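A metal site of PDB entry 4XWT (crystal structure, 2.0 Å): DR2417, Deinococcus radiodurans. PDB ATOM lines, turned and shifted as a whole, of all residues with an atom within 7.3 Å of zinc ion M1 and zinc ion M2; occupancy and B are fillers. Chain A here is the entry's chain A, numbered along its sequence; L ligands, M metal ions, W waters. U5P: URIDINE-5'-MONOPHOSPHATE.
Residues that only touch zinc ion M2: Asn 33. Of the 24 residues printed, 6 come within 4 Å of zinc ion M2. The nearest printed residue that does not touch zinc ion M2 is His 381 (4.5 Å).
Zinc ion M1 is bound by ND1 of His 86 (2.1 Å), NE2 of His 153 (2.3 Å), NE2 of His 84 (2.4 Å) and OD2 of Asp 175 (2.4 Å). Zinc ion M1 has four donor atoms within binding distance.
A ring nitrogen (ND1) of His 403 sits at hydrogen-bond distance from the side-chain hydroxyl (OG1) of Thr 211 (3.0 Å). NE2 of His 89 sits close to ND2 of Asn 33 (3.4 Å). The side-chain carboxylate (OD2) of Asp 47 is in hydrogen-bond range of a ring nitrogen (ND1) of His 89, at 2.8 Å. O of Asp 175 sits at hydrogen-bond distance from ND2 of Asn 158, at 2.8 Å. ND1 of His 153 sits at hydrogen-bond distance from O of Gly 380 (2.8 Å). O of Asp 88 is in hydrogen-bond range of N of Asn 33 (3.0 Å). The side-chain amide oxygen (OD1) of Asn 158 sits close to a ring nitrogen (ND1) of His 84. ND1 of His 84 lies within hydrogen-bond range of OG1 of Thr 83 (2.7 Å).
Zinc ion M2 is bound by NE2 of His 403, at 2.1 Å. Zinc ion M2 is bound by NE2 of His 89, 2.1 Å away. The side-chain carboxylate (OD2) of Asp 175 is bound to zinc ion M2, at 2.2 Å. Zinc ion M2 is bound by OD2 of Asp 88 (2.3 Å). Zinc ion M2 has four donor atoms within binding distance.
An oxygen (O3P) of the ligand lies close to a ring nitrogen (NE2) of His 381, 3.5 Å away. OG of Ser 154 is in hydrogen-bond range of O3P of the ligand. The backbone NH of Gly 380 sits at hydrogen-bond distance from an oxygen (O1P) of the ligand, 2.5 Å away.
Of the 24 residues printed, 4 come within 4 Å of zinc ion M1. The nearest printed residue that does not touch zinc ion M1 is His 89 (4.04 Å).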
ATOM      1  N   ILE A  30      -4.577   3.575  21.673  1.00  0.00           N
ATOM      2  CA  ILE A  30      -5.833   2.870  21.734  1.00  0.00           C
ATOM      3  C   ILE A  30      -6.230   2.752  23.203  1.00  0.00           C
ATOM      4  O   ILE A  30      -5.707   1.911  23.936  1.00  0.00           O
ATOM      5  CB  ILE A  30      -5.728   1.516  21.053  1.00  0.00           C
ATOM      6  CG1 ILE A  30      -5.397   1.719  19.577  1.00  0.00           C
ATOM      7  CG2 ILE A  30      -7.033   0.784  21.151  1.00  0.00           C
ATOM      8  CD1 ILE A  30      -5.354   0.435  18.794  1.00  0.00           C
ATOM      9  N   GLY A  31      -7.135   3.623  23.661  1.00  0.00           N
ATOM     10  CA  GLY A  31      -7.450   3.661  25.082  1.00  0.00           C
ATOM     11  C   GLY A  31      -7.740   5.042  25.660  1.00  0.00           C
ATOM     12  O   GLY A  31      -7.443   6.064  25.034  1.00  0.00           O
ATOM     13  N   ASN A  33     -10.297   7.029  25.866  1.00  0.00           N
ATOM     14  CA  ASN A  33     -10.958   7.995  25.002  1.00  0.00           C
ATOM     15  C   ASN A  33     -11.744   9.072  25.760  1.00  0.00           C
ATOM     16  O   ASN A  33     -12.570   8.782  26.633  1.00  0.00           O
ATOM     17  CB  ASN A  33     -11.862   7.243  24.020  1.00  0.00           C
ATOM     18  CG  ASN A  33     -11.056   6.340  23.085  1.00  0.00           C
ATOM     19  OD1 ASN A  33     -10.417   6.816  22.145  1.00  0.00           O
ATOM     20  ND2 ASN A  33     -11.060   5.034  23.378  1.00  0.00           N
ATOM     21  N   ASP A  47     -17.306  10.706  25.979  1.00  0.00           N
ATOM     22  CA  ASP A  47     -16.665   9.572  26.674  1.00  0.00           C
ATOM     23  C   ASP A  47     -15.672   9.998  27.760  1.00  0.00           C
ATOM     24  O   ASP A  47     -15.438  11.196  27.993  1.00  0.00           O
ATOM     25  CB  ASP A  47     -15.999   8.635  25.642  1.00  0.00           C
ATOM     26  CG  ASP A  47     -17.023   7.919  24.765  1.00  0.00           C
ATOM     27  OD1 ASP A  47     -18.202   7.888  25.168  1.00  0.00           O
ATOM     28  OD2 ASP A  47     -16.674   7.391  23.677  1.00  0.00           O
ATOM     29  N   THR A  83     -20.693   7.089  24.021  1.00  0.00           N
ATOM     30  CA  THR A  83     -20.943   6.360  22.791  1.00  0.00           C
ATOM     31  C   THR A  83     -21.223   4.862  22.997  1.00  0.00           C
ATOM     32  O   THR A  83     -22.047   4.278  22.297  1.00  0.00           O
ATOM     33  CB  THR A  83     -19.762   6.478  21.815  1.00  0.00           C
ATOM     34  OG1 THR A  83     -18.611   5.808  22.381  1.00  0.00           O
ATOM     35  CG2 THR A  83     -19.418   7.936  21.557  1.00  0.00           C
ATOM     36  N   HIS A  84     -20.491   4.237  23.931  1.00  0.00           N
ATOM     37  CA  HIS A  84     -20.745   2.845  24.291  1.00  0.00           C
ATOM     38  C   HIS A  84     -20.042   2.444  25.590  1.00  0.00           C
ATOM     39  O   HIS A  84     -19.255   3.201  26.144  1.00  0.00           O
ATOM     40  CB  HIS A  84     -20.342   1.889  23.154  1.00  0.00           C
ATOM     41  CG  HIS A  84     -18.882   1.939  22.806  1.00  0.00           C
ATOM     42  ND1 HIS A  84     -18.247   3.107  22.440  1.00  0.00           N
ATOM     43  CD2 HIS A  84     -17.946   0.956  22.720  1.00  0.00           C
ATOM     44  CE1 HIS A  84     -16.981   2.844  22.152  1.00  0.00           C
ATOM     45  NE2 HIS A  84     -16.770   1.558  22.333  1.00  0.00           N
ATOM     46  N   GLY A  85     -20.340   1.242  26.067  1.00  0.00           N
ATOM     47  CA  GLY A  85     -19.971   0.853  27.407  1.00  0.00           C
ATOM     48  C   GLY A  85     -18.625   0.135  27.547  1.00  0.00           C
ATOM     49  O   GLY A  85     -18.396  -0.488  28.559  1.00  0.00           O
ATOM     50  N   HIS A  86     -17.750   0.227  26.548  1.00  0.00           N
ATOM     51  CA  HIS A  86     -16.414  -0.378  26.698  1.00  0.00           C
ATOM     52  C   HIS A  86     -15.568   0.389  27.717  1.00  0.00           C
ATOM     53  O   HIS A  86     -15.782   1.579  27.947  1.00  0.00           O
ATOM     54  CB  HIS A  86     -15.678  -0.424  25.361  1.00  0.00           C
ATOM     55  CG  HIS A  86     -16.011  -1.619  24.550  1.00  0.00           C
ATOM     56  ND1 HIS A  86     -15.920  -1.642  23.176  1.00  0.00           N
ATOM     57  CD2 HIS A  86     -16.468  -2.843  24.910  1.00  0.00           C
ATOM     58  CE1 HIS A  86     -16.285  -2.840  22.732  1.00  0.00           C
ATOM     59  NE2 HIS A  86     -16.628  -3.579  23.764  1.00  0.00           N
ATOM     60  N   GLU A  87     -14.591  -0.298  28.324  1.00  0.00           N
ATOM     61  CA  GLU A  87     -13.828   0.329  29.396  1.00  0.00           C
ATOM     62  C   GLU A  87     -13.014   1.519  28.907  1.00  0.00           C
ATOM     63  O   GLU A  87     -12.799   2.468  29.652  1.00  0.00           O
ATOM     64  CB  GLU A  87     -12.906  -0.698  30.071  1.00  0.00           C
ATOM     65  CG  GLU A  87     -13.595  -1.694  30.984  1.00  0.00           C
ATOM     66  CD  GLU A  87     -13.681  -1.209  32.420  1.00  0.00           C
ATOM     67  OE1 GLU A  87     -14.304  -0.154  32.644  1.00  0.00           O
ATOM     68  OE2 GLU A  87     -13.100  -1.879  33.320  1.00  0.00           O
ATOM     69  N   ASP A  88     -12.520   1.487  27.667  1.00  0.00           N
ATOM     70  CA  ASP A  88     -11.787   2.659  27.200  1.00  0.00           C
ATOM     71  C   ASP A  88     -12.701   3.837  26.792  1.00  0.00           C
ATOM     72  O   ASP A  88     -12.230   4.779  26.159  1.00  0.00           O
ATOM     73  CB  ASP A  88     -10.865   2.296  26.020  1.00  0.00           C
ATOM     74  CG  ASP A  88     -11.612   1.650  24.883  1.00  0.00           C
ATOM     75  OD1 ASP A  88     -12.424   0.743  25.164  1.00  0.00           O
ATOM     76  OD2 ASP A  88     -11.376   2.022  23.714  1.00  0.00           O
ATOM     77  N   HIS A  89     -13.990   3.786  27.183  1.00  0.00           N
ATOM     78  CA  HIS A  89     -14.914   4.916  26.961  1.00  0.00           C
ATOM     79  C   HIS A  89     -15.669   5.318  28.227  1.00  0.00           C
ATOM     80  O   HIS A  89     -16.029   6.482  28.371  1.00  0.00           O
ATOM     81  CB  HIS A  89     -15.879   4.603  25.805  1.00  0.00           C
ATOM     82  CG  HIS A  89     -15.168   4.284  24.525  1.00  0.00           C
ATOM     83  ND1 HIS A  89     -15.005   5.202  23.514  1.00  0.00           N
ATOM     84  CD2 HIS A  89     -14.475   3.180  24.140  1.00  0.00           C
ATOM     85  CE1 HIS A  89     -14.300   4.669  22.542  1.00  0.00           C
ATOM     86  NE2 HIS A  89     -13.970   3.428  22.889  1.00  0.00           N
ATOM     87  N   HIS A 153     -20.895  -2.660  16.450  1.00  0.00           N
ATOM     88  CA  HIS A 153     -19.585  -2.759  17.089  1.00  0.00           C
ATOM     89  C   HIS A 153     -19.557  -4.096  17.835  1.00  0.00           C
ATOM     90  O   HIS A 153     -20.407  -4.950  17.579  1.00  0.00           O
ATOM     91  CB  HIS A 153     -19.376  -1.514  18.001  1.00  0.00           C
ATOM     92  CG  HIS A 153     -18.037  -1.441  18.661  1.00  0.00           C
ATOM     93  ND1 HIS A 153     -16.866  -1.851  18.045  1.00  0.00           N
ATOM     94  CD2 HIS A 153     -17.673  -0.998  19.884  1.00  0.00           C
ATOM     95  CE1 HIS A 153     -15.847  -1.672  18.864  1.00  0.00           C
ATOM     96  NE2 HIS A 153     -16.307  -1.158  19.993  1.00  0.00           N
ATOM     97  N   SER A 154     -18.602  -4.310  18.732  1.00  0.00           N
ATOM     98  CA  SER A 154     -18.485  -5.581  19.459  1.00  0.00           C
ATOM     99  C   SER A 154     -19.253  -5.562  20.783  1.00  0.00           C
ATOM    100  O   SER A 154     -19.166  -6.502  21.596  1.00  0.00           O
ATOM    101  CB  SER A 154     -17.013  -5.899  19.721  1.00  0.00           C
ATOM    102  OG  SER A 154     -16.473  -4.791  20.426  1.00  0.00           O
ATOM    103  N   ILE A 155     -19.996  -4.473  21.013  1.00  0.00           N
ATOM    104  CA  ILE A 155     -20.915  -4.377  22.150  1.00  0.00           C
ATOM    105  C   ILE A 155     -22.226  -3.728  21.656  1.00  0.00           C
ATOM    106  O   ILE A 155     -22.201  -2.879  20.771  1.00  0.00           O
ATOM    107  CB  ILE A 155     -20.299  -3.573  23.344  1.00  0.00           C
ATOM    108  CG1 ILE A 155     -21.066  -3.847  24.645  1.00  0.00           C
ATOM    109  CG2 ILE A 155     -20.228  -2.065  23.027  1.00  0.00           C
ATOM    110  CD1 ILE A 155     -20.525  -3.137  25.918  1.00  0.00           C
ATOM    111  N   ASN A 158     -24.251   0.795  20.752  1.00  0.00           N
ATOM    112  CA  ASN A 158     -23.059   1.529  20.393  1.00  0.00           C
ATOM    113  C   ASN A 158     -23.470   2.573  19.398  1.00  0.00           C
ATOM    114  O   ASN A 158     -24.166   2.255  18.430  1.00  0.00           O
ATOM    115  CB  ASN A 158     -22.017   0.573  19.829  1.00  0.00           C
ATOM    116  CG  ASN A 158     -20.827   1.268  19.251  1.00  0.00           C
ATOM    117  OD1 ASN A 158     -19.892   1.632  19.968  1.00  0.00           O
ATOM    118  ND2 ASN A 158     -20.823   1.432  17.942  1.00  0.00           N
ATOM    119  N   GLY A 174     -17.859   7.036  16.227  1.00  0.00           N
ATOM    120  CA  GLY A 174     -17.661   6.241  17.407  1.00  0.00           C
ATOM    121  C   GLY A 174     -16.783   5.055  17.021  1.00  0.00           C
ATOM    122  O   GLY A 174     -16.127   5.072  15.978  1.00  0.00           O
ATOM    123  N   ASP A 175     -16.741   4.036  17.876  1.00  0.00           N
ATOM    124  CA  ASP A 175     -16.168   2.742  17.507  1.00  0.00           C
ATOM    125  C   ASP A 175     -17.091   2.034  16.538  1.00  0.00           C
ATOM    126  O   ASP A 175     -18.303   1.998  16.777  1.00  0.00           O
ATOM    127  CB  ASP A 175     -15.976   1.853  18.744  1.00  0.00           C
ATOM    128  CG  ASP A 175     -14.838   2.298  19.642  1.00  0.00           C
ATOM    129  OD1 ASP A 175     -14.535   3.528  19.675  1.00  0.00           O
ATOM    130  OD2 ASP A 175     -14.278   1.393  20.319  1.00  0.00           O
ATOM    131  N   PHE A 176     -16.558   1.455  15.462  1.00  0.00           N
ATOM    132  CA  PHE A 176     -17.426   0.709  14.554  1.00  0.00           C
ATOM    133  C   PHE A 176     -16.756  -0.321  13.664  1.00  0.00           C
ATOM    134  O   PHE A 176     -15.574  -0.225  13.337  1.00  0.00           O
ATOM    135  CB  PHE A 176     -18.170   1.667  13.633  1.00  0.00           C
ATOM    136  CG  PHE A 176     -17.381   2.124  12.438  1.00  0.00           C
ATOM    137  CD1 PHE A 176     -16.451   3.144  12.567  1.00  0.00           C
ATOM    138  CD2 PHE A 176     -17.609   1.584  11.181  1.00  0.00           C
ATOM    139  CE1 PHE A 176     -15.747   3.600  11.468  1.00  0.00           C
ATOM    140  CE2 PHE A 176     -16.901   2.033  10.049  1.00  0.00           C
ATOM    141  CZ  PHE A 176     -15.961   3.046  10.199  1.00  0.00           C
ATOM    142  N   ASP A 209     -12.870   5.857  13.451  1.00  0.00           N
ATOM    143  CA  ASP A 209     -12.190   4.814  14.190  1.00  0.00           C
ATOM    144  C   ASP A 209     -11.052   4.182  13.384  1.00  0.00           C
ATOM    145  O   ASP A 209     -11.307   3.556  12.364  1.00  0.00           O
ATOM    146  CB  ASP A 209     -13.225   3.759  14.596  1.00  0.00           C
ATOM    147  CG  ASP A 209     -12.623   2.545  15.287  1.00  0.00           C
ATOM    148  OD1 ASP A 209     -11.414   2.516  15.592  1.00  0.00           O
ATOM    149  OD2 ASP A 209     -13.396   1.607  15.554  1.00  0.00           O
ATOM    150  N   THR A 211      -8.616   1.897  14.417  1.00  0.00           N
ATOM    151  CA  THR A 211      -8.021   0.720  15.053  1.00  0.00           C
ATOM    152  C   THR A 211      -7.430  -0.244  14.034  1.00  0.00           C
ATOM    153  O   THR A 211      -6.282  -0.690  14.158  1.00  0.00           O
ATOM    154  CB  THR A 211      -9.050  -0.051  15.903  1.00  0.00           C
ATOM    155  OG1 THR A 211      -9.608   0.819  16.900  1.00  0.00           O
ATOM    156  CG2 THR A 211      -8.386  -1.241  16.587  1.00  0.00           C
ATOM    157  N   GLY A 380     -13.935  -5.967  16.547  1.00  0.00           N
ATOM    158  CA  GLY A 380     -15.055  -5.051  16.641  1.00  0.00           C
ATOM    159  C   GLY A 380     -14.891  -3.818  15.766  1.00  0.00           C
ATOM    160  O   GLY A 380     -15.764  -2.963  15.753  1.00  0.00           O
ATOM    161  N   HIS A 381     -13.801  -3.771  15.011  1.00  0.00           N
ATOM    162  CA  HIS A 381     -13.438  -2.555  14.297  1.00  0.00           C
ATOM    163  C   HIS A 381     -13.342  -2.752  12.793  1.00  0.00           C
ATOM    164  O   HIS A 381     -12.876  -3.781  12.302  1.00  0.00           O
ATOM    165  CB  HIS A 381     -12.108  -2.009  14.831  1.00  0.00           C
ATOM    166  CG  HIS A 381     -12.169  -1.635  16.275  1.00  0.00           C
ATOM    167  ND1 HIS A 381     -12.424  -0.340  16.704  1.00  0.00           N
ATOM    168  CD2 HIS A 381     -12.019  -2.365  17.405  1.00  0.00           C
ATOM    169  CE1 HIS A 381     -12.418  -0.304  18.019  1.00  0.00           C
ATOM    170  NE2 HIS A 381     -12.171  -1.527  18.476  1.00  0.00           N
ATOM    171  N   TRP A 402      -8.836   8.930  14.304  1.00  0.00           N
ATOM    172  CA  TRP A 402      -8.895   8.876  15.761  1.00  0.00           C
ATOM    173  C   TRP A 402      -8.921   7.408  16.249  1.00  0.00           C
ATOM    174  O   TRP A 402      -8.978   6.498  15.415  1.00  0.00           O
ATOM    175  CB  TRP A 402     -10.132   9.695  16.214  1.00  0.00           C
ATOM    176  CG  TRP A 402     -10.744   9.312  17.501  1.00  0.00           C
ATOM    177  CD1 TRP A 402     -10.405   9.792  18.720  1.00  0.00           C
ATOM    178  CD2 TRP A 402     -11.792   8.347  17.704  1.00  0.00           C
ATOM    179  NE1 TRP A 402     -11.181   9.190  19.683  1.00  0.00           N
ATOM    180  CE2 TRP A 402     -12.028   8.292  19.086  1.00  0.00           C
ATOM    181  CE3 TRP A 402     -12.527   7.518  16.857  1.00  0.00           C
ATOM    182  CZ2 TRP A 402     -12.985   7.442  19.650  1.00  0.00           C
ATOM    183  CZ3 TRP A 402     -13.483   6.673  17.409  1.00  0.00           C
ATOM    184  CH2 TRP A 402     -13.715   6.659  18.798  1.00  0.00           C
ATOM    185  N   HIS A 403      -8.851   7.153  17.564  1.00  0.00           N
ATOM    186  CA  HIS A 403      -8.862   5.799  18.163  1.00  0.00           C
ATOM    187  C   HIS A 403      -7.777   4.902  17.543  1.00  0.00           C
ATOM    188  O   HIS A 403      -8.051   3.818  17.052  1.00  0.00           O
ATOM    189  CB  HIS A 403     -10.256   5.122  18.006  1.00  0.00           C
ATOM    190  CG  HIS A 403     -10.599   4.084  19.051  1.00  0.00           C
ATOM    191  ND1 HIS A 403     -10.039   2.827  19.094  1.00  0.00           N
ATOM    192  CD2 HIS A 403     -11.510   4.120  20.061  1.00  0.00           C
ATOM    193  CE1 HIS A 403     -10.585   2.134  20.088  1.00  0.00           C
ATOM    194  NE2 HIS A 403     -11.481   2.899  20.690  1.00  0.00           N
HETATM  195  N1  U5P L   1     -10.147  -4.522  23.025  1.00  0.00           N
HETATM  196  C2  U5P L   1     -10.235  -4.176  24.387  1.00  0.00           C
HETATM  197  N3  U5P L   1     -11.347  -4.435  25.079  1.00  0.00           N
HETATM  198  C4  U5P L   1     -12.395  -5.017  24.496  1.00  0.00           C
HETATM  199  C5  U5P L   1     -12.342  -5.363  23.145  1.00  0.00           C
HETATM  200  C6  U5P L   1     -11.193  -5.100  22.429  1.00  0.00           C
HETATM  201  O2  U5P L   1      -9.266  -3.621  24.950  1.00  0.00           O
HETATM  202  O4  U5P L   1     -13.410  -5.248  25.157  1.00  0.00           O
HETATM  203  C1' U5P L   1      -8.923  -4.226  22.261  1.00  0.00           C
HETATM  204  C2' U5P L   1      -8.453  -5.439  21.478  1.00  0.00           C
HETATM  205  O2' U5P L   1      -7.305  -6.029  22.095  1.00  0.00           O
HETATM  206  C3' U5P L   1      -8.096  -4.899  20.111  1.00  0.00           C
HETATM  207  C4' U5P L   1      -8.917  -3.642  19.977  1.00  0.00           C
HETATM  208  O3' U5P L   1      -6.716  -4.526  20.067  1.00  0.00           O
HETATM  209  O4' U5P L   1      -9.199  -3.202  21.305  1.00  0.00           O
HETATM  210  C5' U5P L   1     -10.218  -3.945  19.262  1.00  0.00           C
HETATM  211  O5' U5P L   1     -10.766  -5.168  19.762  1.00  0.00           O
HETATM  212  P   U5P L   1     -12.135  -5.745  19.152  1.00  0.00           P
HETATM  213  O1P U5P L   1     -11.752  -5.858  17.711  1.00  0.00           O
HETATM  214  O2P U5P L   1     -12.391  -7.052  19.861  1.00  0.00           O
HETATM  215  O3P U5P L   1     -13.159  -4.703  19.491  1.00  0.00           O
HETATM  216 ZN    ZN M   1     -15.281  -0.230  21.794  1.00  0.00          ZN
HETATM  217 ZN    ZN M   2     -12.841   1.957  21.908  1.00  0.00          ZN
HETATM  218  O   HOH W   1     -12.466  -1.576  21.494  1.00  0.00           O
